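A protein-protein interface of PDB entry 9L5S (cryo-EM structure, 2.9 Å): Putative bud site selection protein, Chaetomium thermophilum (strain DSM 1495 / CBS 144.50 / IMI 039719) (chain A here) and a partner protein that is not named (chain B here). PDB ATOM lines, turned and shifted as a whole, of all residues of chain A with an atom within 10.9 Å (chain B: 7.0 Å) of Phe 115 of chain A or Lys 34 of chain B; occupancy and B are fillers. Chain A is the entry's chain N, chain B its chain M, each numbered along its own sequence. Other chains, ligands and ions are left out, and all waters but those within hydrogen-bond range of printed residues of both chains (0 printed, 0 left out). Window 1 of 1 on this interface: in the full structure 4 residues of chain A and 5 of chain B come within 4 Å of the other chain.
The backbone carbonyl oxygen of Ser 55 of chain B sits at hydrogen-bond distance from the backbone NH of Leu 36 of chain B, 2.9 Å away.
ND2 of Asn 114 of chain A touches CD1 of Leu 36 of chain B, 3.6 Å away.
Phe 115 of chain A touches Lys 34 of chain B (CZ to C, 3.4 Å).
Met 35 of chain B touches Phe 115 of chain A (N to CE1, 3.4 Å).
Phe 115 of chain A touches Leu 36 of chain B.
Ile 120 of chain A touches Arg 61 of chain B (CD1 to CZ, 3.8 Å).
Of the printed residues of chain B, Asn 114 of chain A touches Leu 36.
Phe 115 of chain A touches just these residues of chain B: Lys 34, Met 35 and Leu 36.
Of the printed residues of chain B, Ile 120 of chain A touches Arg 61 (3.8 Å).
Val 33 of chain B touches none of the printed residues of chain A.
Lys 34 of chain B touches just one residue of chain A: Phe 115 (3.4 Å).
Of the printed residues of chain A, Met 35 of chain B touches Phe 115.
Of chain A, only Asn 114 and Phe 115 come within 4 Å of Leu 36 of chain B.
Trp 56 of chain B touches none of the printed residues of chain A.
No residue of chain A comes within 4 Å of Ala 57 of chain B.
The nearest residue of chain B that does not touch Phe 115 of chain A is Ser 55 of chain B (5.4 Å).
The nearest printed residue of chain A that does not touch Arg 61 of chain B is Val 123 of chain A (7.8 Å).
Hydrophobic or aromatic side chains of chain B within 4 Å of the printed part of chain A: Leu 36.
Of the 13 printed residues of chain A, 3 touch a printed residue of chain B.
Among the printed residues, 5 pairs touch across the chains.
Among the printed residues, no Asp or Glu carboxylate lies within 4 Å of a Lys or Arg side-chain nitrogen of the other chain.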
ATOM      1  N   GLN A 109       0.833 -33.585 -18.892  1.00  0.00           N
ATOM      2  CA  GLN A 109       0.516 -32.664 -17.804  1.00  0.00           C
ATOM      3  C   GLN A 109      -0.257 -31.497 -18.402  1.00  0.00           C
ATOM      4  O   GLN A 109       0.316 -30.504 -18.850  1.00  0.00           O
ATOM      5  CB  GLN A 109       1.785 -32.200 -17.101  1.00  0.00           C
ATOM      6  CG  GLN A 109       1.530 -31.408 -15.834  1.00  0.00           C
ATOM      7  CD  GLN A 109       0.496 -32.062 -14.944  1.00  0.00           C
ATOM      8  OE1 GLN A 109      -0.591 -31.526 -14.742  1.00  0.00           O
ATOM      9  NE2 GLN A 109       0.828 -33.228 -14.409  1.00  0.00           N
ATOM     10  N   THR A 110      -1.585 -31.624 -18.410  1.00  0.00           N
ATOM     11  CA  THR A 110      -2.430 -30.622 -19.044  1.00  0.00           C
ATOM     12  C   THR A 110      -2.542 -29.346 -18.226  1.00  0.00           C
ATOM     13  O   THR A 110      -2.838 -28.290 -18.791  1.00  0.00           O
ATOM     14  CB  THR A 110      -3.823 -31.191 -19.295  1.00  0.00           C
ATOM     15  OG1 THR A 110      -4.310 -31.806 -18.097  1.00  0.00           O
ATOM     16  CG2 THR A 110      -3.783 -32.215 -20.405  1.00  0.00           C
ATOM     17  N   LYS A 111      -2.302 -29.408 -16.920  1.00  0.00           N
ATOM     18  CA  LYS A 111      -2.388 -28.223 -16.078  1.00  0.00           C
ATOM     19  C   LYS A 111      -1.234 -27.253 -16.292  1.00  0.00           C
ATOM     20  O   LYS A 111      -1.283 -26.138 -15.766  1.00  0.00           O
ATOM     21  CB  LYS A 111      -2.447 -28.626 -14.603  1.00  0.00           C
ATOM     22  CG  LYS A 111      -3.765 -29.249 -14.178  1.00  0.00           C
ATOM     23  CD  LYS A 111      -3.735 -29.654 -12.712  1.00  0.00           C
ATOM     24  CE  LYS A 111      -2.925 -30.923 -12.509  1.00  0.00           C
ATOM     25  NZ  LYS A 111      -2.963 -31.404 -11.102  1.00  0.00           N
ATOM     26  N   GLU A 112      -0.208 -27.643 -17.048  1.00  0.00           N
ATOM     27  CA  GLU A 112       1.009 -26.853 -17.176  1.00  0.00           C
ATOM     28  C   GLU A 112       1.289 -26.421 -18.612  1.00  0.00           C
ATOM     29  O   GLU A 112       2.434 -26.101 -18.946  1.00  0.00           O
ATOM     30  CB  GLU A 112       2.192 -27.632 -16.607  1.00  0.00           C
ATOM     31  CG  GLU A 112       2.229 -27.597 -15.097  1.00  0.00           C
ATOM     32  CD  GLU A 112       3.237 -28.550 -14.512  1.00  0.00           C
ATOM     33  OE1 GLU A 112       4.278 -28.793 -15.156  1.00  0.00           O
ATOM     34  OE2 GLU A 112       2.988 -29.045 -13.399  1.00  0.00           O
ATOM     35  N   THR A 113       0.275 -26.406 -19.466  1.00  0.00           N
ATOM     36  CA  THR A 113       0.377 -25.820 -20.792  1.00  0.00           C
ATOM     37  C   THR A 113      -0.405 -24.514 -20.830  1.00  0.00           C
ATOM     38  O   THR A 113      -1.146 -24.185 -19.899  1.00  0.00           O
ATOM     39  CB  THR A 113      -0.135 -26.781 -21.870  1.00  0.00           C
ATOM     40  OG1 THR A 113      -1.364 -27.372 -21.440  1.00  0.00           O
ATOM     41  CG2 THR A 113       0.885 -27.877 -22.132  1.00  0.00           C
ATOM     42  N   ASN A 114      -0.213 -23.761 -21.917  1.00  0.00           N
ATOM     43  CA  ASN A 114      -0.834 -22.445 -22.039  1.00  0.00           C
ATOM     44  C   ASN A 114      -2.352 -22.548 -22.125  1.00  0.00           C
ATOM     45  O   ASN A 114      -3.075 -21.784 -21.476  1.00  0.00           O
ATOM     46  CB  ASN A 114      -0.282 -21.711 -23.262  1.00  0.00           C
ATOM     47  CG  ASN A 114       1.152 -21.256 -23.075  1.00  0.00           C
ATOM     48  OD1 ASN A 114       1.548 -20.849 -21.985  1.00  0.00           O
ATOM     49  ND2 ASN A 114       1.934 -21.309 -24.146  1.00  0.00           N
ATOM     50  N   PHE A 115      -2.855 -23.492 -22.918  1.00  0.00           N
ATOM     51  CA  PHE A 115      -4.282 -23.620 -23.181  1.00  0.00           C
ATOM     52  C   PHE A 115      -4.837 -24.953 -22.693  1.00  0.00           C
ATOM     53  O   PHE A 115      -5.836 -25.444 -23.226  1.00  0.00           O
ATOM     54  CB  PHE A 115      -4.560 -23.423 -24.668  1.00  0.00           C
ATOM     55  CG  PHE A 115      -4.074 -22.106 -25.190  1.00  0.00           C
ATOM     56  CD1 PHE A 115      -4.736 -20.935 -24.866  1.00  0.00           C
ATOM     57  CD2 PHE A 115      -2.941 -22.036 -25.983  1.00  0.00           C
ATOM     58  CE1 PHE A 115      -4.284 -19.720 -25.333  1.00  0.00           C
ATOM     59  CE2 PHE A 115      -2.485 -20.823 -26.454  1.00  0.00           C
ATOM     60  CZ  PHE A 115      -3.157 -19.664 -26.128  1.00  0.00           C
ATOM     61  N   ASN A 116      -4.184 -25.535 -21.683  1.00  0.00           N
ATOM     62  CA  ASN A 116      -4.603 -26.781 -21.034  1.00  0.00           C
ATOM     63  C   ASN A 116      -4.690 -27.936 -22.027  1.00  0.00           C
ATOM     64  O   ASN A 116      -5.619 -28.745 -22.002  1.00  0.00           O
ATOM     65  CB  ASN A 116      -5.919 -26.596 -20.281  1.00  0.00           C
ATOM     66  CG  ASN A 116      -5.792 -25.630 -19.124  1.00  0.00           C
ATOM     67  OD1 ASN A 116      -6.593 -24.708 -18.977  1.00  0.00           O
ATOM     68  ND2 ASN A 116      -4.782 -25.838 -18.290  1.00  0.00           N
ATOM     69  N   SER A 117      -3.706 -28.009 -22.913  1.00  0.00           N
ATOM     70  CA  SER A 117      -3.593 -29.080 -23.887  1.00  0.00           C
ATOM     71  C   SER A 117      -2.569 -30.110 -23.426  1.00  0.00           C
ATOM     72  O   SER A 117      -1.816 -29.898 -22.475  1.00  0.00           O
ATOM     73  CB  SER A 117      -3.202 -28.514 -25.256  1.00  0.00           C
ATOM     74  OG  SER A 117      -3.956 -27.356 -25.568  1.00  0.00           O
ATOM     75  N   THR A 118      -2.551 -31.243 -24.120  1.00  0.00           N
ATOM     76  CA  THR A 118      -1.437 -32.173 -24.010  1.00  0.00           C
ATOM     77  C   THR A 118      -0.337 -31.692 -24.951  1.00  0.00           C
ATOM     78  O   THR A 118      -0.422 -30.616 -25.547  1.00  0.00           O
ATOM     79  CB  THR A 118      -1.866 -33.599 -24.341  1.00  0.00           C
ATOM     80  OG1 THR A 118      -2.185 -33.688 -25.734  1.00  0.00           O
ATOM     81  CG2 THR A 118      -3.073 -34.007 -23.524  1.00  0.00           C
ATOM     82  N   CYS A 119       0.711 -32.487 -25.105  1.00  0.00           N
ATOM     83  CA  CYS A 119       1.704 -32.144 -26.103  1.00  0.00           C
ATOM     84  C   CYS A 119       1.193 -32.472 -27.503  1.00  0.00           C
ATOM     85  O   CYS A 119       0.284 -33.285 -27.691  1.00  0.00           O
ATOM     86  CB  CYS A 119       3.013 -32.875 -25.843  1.00  0.00           C
ATOM     87  SG  CYS A 119       4.360 -32.130 -26.742  1.00  0.00           S
ATOM     88  N   ILE A 120       1.797 -31.816 -28.497  1.00  0.00           N
ATOM     89  CA  ILE A 120       1.453 -32.074 -29.890  1.00  0.00           C
ATOM     90  C   ILE A 120       1.903 -33.462 -30.335  1.00  0.00           C
ATOM     91  O   ILE A 120       1.404 -33.978 -31.340  1.00  0.00           O
ATOM     92  CB  ILE A 120       2.041 -30.962 -30.785  1.00  0.00           C
ATOM     93  CG1 ILE A 120       1.263 -30.845 -32.099  1.00  0.00           C
ATOM     94  CG2 ILE A 120       3.528 -31.185 -31.040  1.00  0.00           C
ATOM     95  CD1 ILE A 120       1.629 -29.629 -32.913  1.00  0.00           C
ATOM     96  N   VAL A 123      -0.801 -36.381 -30.458  1.00  0.00           N
ATOM     97  CA  VAL A 123      -1.778 -36.367 -31.544  1.00  0.00           C
ATOM     98  C   VAL A 123      -1.475 -37.503 -32.513  1.00  0.00           C
ATOM     99  O   VAL A 123      -0.299 -37.761 -32.810  1.00  0.00           O
ATOM    100  CB  VAL A 123      -1.768 -35.001 -32.251  1.00  0.00           C
ATOM    101  CG1 VAL A 123      -2.798 -34.941 -33.367  1.00  0.00           C
ATOM    102  CG2 VAL A 123      -2.001 -33.902 -31.241  1.00  0.00           C
ATOM    103  N   PRO B  28      -4.777 -15.573 -37.039  1.00  0.00           N
ATOM    104  CA  PRO B  28      -4.668 -16.885 -37.688  1.00  0.00           C
ATOM    105  C   PRO B  28      -5.795 -17.141 -38.678  1.00  0.00           C
ATOM    106  O   PRO B  28      -6.882 -16.569 -38.581  1.00  0.00           O
ATOM    107  CB  PRO B  28      -4.736 -17.865 -36.512  1.00  0.00           C
ATOM    108  CG  PRO B  28      -4.205 -17.099 -35.368  1.00  0.00           C
ATOM    109  CD  PRO B  28      -4.686 -15.691 -35.572  1.00  0.00           C
ATOM    110  N   TYR B  32     -10.971 -19.821 -34.938  1.00  0.00           N
ATOM    111  CA  TYR B  32     -10.980 -20.009 -33.494  1.00  0.00           C
ATOM    112  C   TYR B  32      -9.559 -19.774 -33.005  1.00  0.00           C
ATOM    113  O   TYR B  32      -8.645 -20.533 -33.346  1.00  0.00           O
ATOM    114  CB  TYR B  32     -11.497 -21.402 -33.138  1.00  0.00           C
ATOM    115  CG  TYR B  32     -12.881 -21.647 -33.697  1.00  0.00           C
ATOM    116  CD1 TYR B  32     -14.015 -21.274 -32.991  1.00  0.00           C
ATOM    117  CD2 TYR B  32     -13.052 -22.241 -34.944  1.00  0.00           C
ATOM    118  CE1 TYR B  32     -15.280 -21.484 -33.510  1.00  0.00           C
ATOM    119  CE2 TYR B  32     -14.309 -22.454 -35.469  1.00  0.00           C
ATOM    120  CZ  TYR B  32     -15.420 -22.074 -34.748  1.00  0.00           C
ATOM    121  OH  TYR B  32     -16.675 -22.289 -35.266  1.00  0.00           O
ATOM    122  N   VAL B  33      -9.369 -18.710 -32.232  1.00  0.00           N
ATOM    123  CA  VAL B  33      -8.046 -18.206 -31.887  1.00  0.00           C
ATOM    124  C   VAL B  33      -7.780 -18.507 -30.420  1.00  0.00           C
ATOM    125  O   VAL B  33      -8.554 -18.104 -29.545  1.00  0.00           O
ATOM    126  CB  VAL B  33      -7.926 -16.699 -32.165  1.00  0.00           C
ATOM    127  CG1 VAL B  33      -6.470 -16.264 -32.124  1.00  0.00           C
ATOM    128  CG2 VAL B  33      -8.554 -16.355 -33.505  1.00  0.00           C
ATOM    129  N   LYS B  34      -6.691 -19.219 -30.156  1.00  0.00           N
ATOM    130  CA  LYS B  34      -6.193 -19.409 -28.802  1.00  0.00           C
ATOM    131  C   LYS B  34      -5.168 -18.318 -28.522  1.00  0.00           C
ATOM    132  O   LYS B  34      -4.136 -18.241 -29.196  1.00  0.00           O
ATOM    133  CB  LYS B  34      -5.581 -20.797 -28.641  1.00  0.00           C
ATOM    134  CG  LYS B  34      -6.575 -21.927 -28.825  1.00  0.00           C
ATOM    135  CD  LYS B  34      -6.001 -23.246 -28.348  1.00  0.00           C
ATOM    136  CE  LYS B  34      -4.867 -23.702 -29.247  1.00  0.00           C
ATOM    137  NZ  LYS B  34      -4.528 -25.133 -29.032  1.00  0.00           N
ATOM    138  N   MET B  35      -5.453 -17.473 -27.534  1.00  0.00           N
ATOM    139  CA  MET B  35      -4.697 -16.249 -27.322  1.00  0.00           C
ATOM    140  C   MET B  35      -4.221 -16.164 -25.878  1.00  0.00           C
ATOM    141  O   MET B  35      -4.985 -16.424 -24.945  1.00  0.00           O
ATOM    142  CB  MET B  35      -5.555 -15.027 -27.675  1.00  0.00           C
ATOM    143  CG  MET B  35      -4.836 -13.696 -27.618  1.00  0.00           C
ATOM    144  SD  MET B  35      -5.867 -12.373 -28.280  1.00  0.00           S
ATOM    145  CE  MET B  35      -5.627 -12.598 -30.038  1.00  0.00           C
ATOM    146  N   LEU B  36      -2.951 -15.810 -25.705  1.00  0.00           N
ATOM    147  CA  LEU B  36      -2.363 -15.550 -24.401  1.00  0.00           C
ATOM    148  C   LEU B  36      -2.388 -14.054 -24.121  1.00  0.00           C
ATOM    149  O   LEU B  36      -2.243 -13.241 -25.036  1.00  0.00           O
ATOM    150  CB  LEU B  36      -0.925 -16.068 -24.339  1.00  0.00           C
ATOM    151  CG  LEU B  36      -0.737 -17.578 -24.196  1.00  0.00           C
ATOM    152  CD1 LEU B  36       0.701 -17.960 -24.489  1.00  0.00           C
ATOM    153  CD2 LEU B  36      -1.141 -18.038 -22.808  1.00  0.00           C
ATOM    154  N   LYS B  37      -2.569 -13.695 -22.852  1.00  0.00           N
ATOM    155  CA  LYS B  37      -2.655 -12.301 -22.435  1.00  0.00           C
ATOM    156  C   LYS B  37      -1.757 -12.082 -21.228  1.00  0.00           C
ATOM    157  O   LYS B  37      -1.866 -12.803 -20.231  1.00  0.00           O
ATOM    158  CB  LYS B  37      -4.101 -11.920 -22.102  1.00  0.00           C
ATOM    159  CG  LYS B  37      -4.241 -10.695 -21.219  1.00  0.00           C
ATOM    160  CD  LYS B  37      -5.662 -10.543 -20.714  1.00  0.00           C
ATOM    161  CE  LYS B  37      -5.780  -9.380 -19.745  1.00  0.00           C
ATOM    162  NZ  LYS B  37      -7.191  -9.124 -19.350  1.00  0.00           N
ATOM    163  N   SER B  55      -0.882 -12.367 -27.435  1.00  0.00           N
ATOM    164  CA  SER B  55      -0.027 -13.157 -28.306  1.00  0.00           C
ATOM    165  C   SER B  55      -0.770 -14.401 -28.768  1.00  0.00           C
ATOM    166  O   SER B  55      -1.662 -14.900 -28.083  1.00  0.00           O
ATOM    167  CB  SER B  55       1.282 -13.544 -27.605  1.00  0.00           C
ATOM    168  OG  SER B  55       1.036 -14.334 -26.457  1.00  0.00           O
ATOM    169  N   TRP B  56      -0.402 -14.885 -29.950  1.00  0.00           N
ATOM    170  CA  TRP B  56      -1.065 -16.035 -30.546  1.00  0.00           C
ATOM    171  C   TRP B  56      -0.090 -16.722 -31.488  1.00  0.00           C
ATOM    172  O   TRP B  56       0.911 -16.140 -31.914  1.00  0.00           O
ATOM    173  CB  TRP B  56      -2.337 -15.624 -31.296  1.00  0.00           C
ATOM    174  CG  TRP B  56      -2.075 -14.626 -32.370  1.00  0.00           C
ATOM    175  CD1 TRP B  56      -1.837 -14.885 -33.687  1.00  0.00           C
ATOM    176  CD2 TRP B  56      -2.003 -13.205 -32.221  1.00  0.00           C
ATOM    177  NE1 TRP B  56      -1.629 -13.713 -34.369  1.00  0.00           N
ATOM    178  CE2 TRP B  56      -1.724 -12.667 -33.491  1.00  0.00           C
ATOM    179  CE3 TRP B  56      -2.151 -12.336 -31.137  1.00  0.00           C
ATOM    180  CZ2 TRP B  56      -1.590 -11.300 -33.705  1.00  0.00           C
ATOM    181  CZ3 TRP B  56      -2.016 -10.981 -31.352  1.00  0.00           C
ATOM    182  CH2 TRP B  56      -1.738 -10.477 -32.625  1.00  0.00           C
ATOM    183  N   ALA B  57      -0.403 -17.967 -31.826  1.00  0.00           N
ATOM    184  CA  ALA B  57       0.423 -18.764 -32.722  1.00  0.00           C
ATOM    185  C   ALA B  57      -0.106 -18.631 -34.143  1.00  0.00           C
ATOM    186  O   ALA B  57      -1.301 -18.828 -34.388  1.00  0.00           O
ATOM    187  CB  ALA B  57       0.437 -20.232 -32.296  1.00  0.00           C
ATOM    188  N   ARG B  61       2.512 -23.494 -38.357  1.00  0.00           N
ATOM    189  CA  ARG B  61       2.526 -24.454 -37.262  1.00  0.00           C
ATOM    190  C   ARG B  61       3.909 -25.073 -37.067  1.00  0.00           C
ATOM    191  O   ARG B  61       4.648 -25.293 -38.032  1.00  0.00           O
ATOM    192  CB  ARG B  61       1.471 -25.536 -37.526  1.00  0.00           C
ATOM    193  CG  ARG B  61       1.577 -26.801 -36.680  1.00  0.00           C
ATOM    194  CD  ARG B  61       0.646 -26.795 -35.478  1.00  0.00           C
ATOM    195  NE  ARG B  61       1.243 -26.118 -34.333  1.00  0.00           N
ATOM    196  CZ  ARG B  61       0.652 -25.971 -33.155  1.00  0.00           C
ATOM    197  NH1 ARG B  61      -0.552 -26.465 -32.920  1.00  0.00           N
ATOM    198  NH2 ARG B  61       1.286 -25.316 -32.188  1.00  0.00           N
ATOM    199  N   LYS B  66       6.045 -16.357 -32.445  1.00  0.00           N
ATOM    200  CA  LYS B  66       4.830 -16.073 -31.689  1.00  0.00           C
ATOM    201  C   LYS B  66       4.408 -14.637 -31.973  1.00  0.00           C
ATOM    202  O   LYS B  66       5.009 -13.694 -31.449  1.00  0.00           O
ATOM    203  CB  LYS B  66       5.088 -16.288 -30.200  1.00  0.00           C
ATOM    204  CG  LYS B  66       3.891 -16.052 -29.295  1.00  0.00           C
ATOM    205  CD  LYS B  66       2.833 -17.125 -29.470  1.00  0.00           C
ATOM    206  CE  LYS B  66       3.278 -18.446 -28.867  1.00  0.00           C
ATOM    207  NZ  LYS B  66       2.209 -19.481 -28.945  1.00  0.00           N
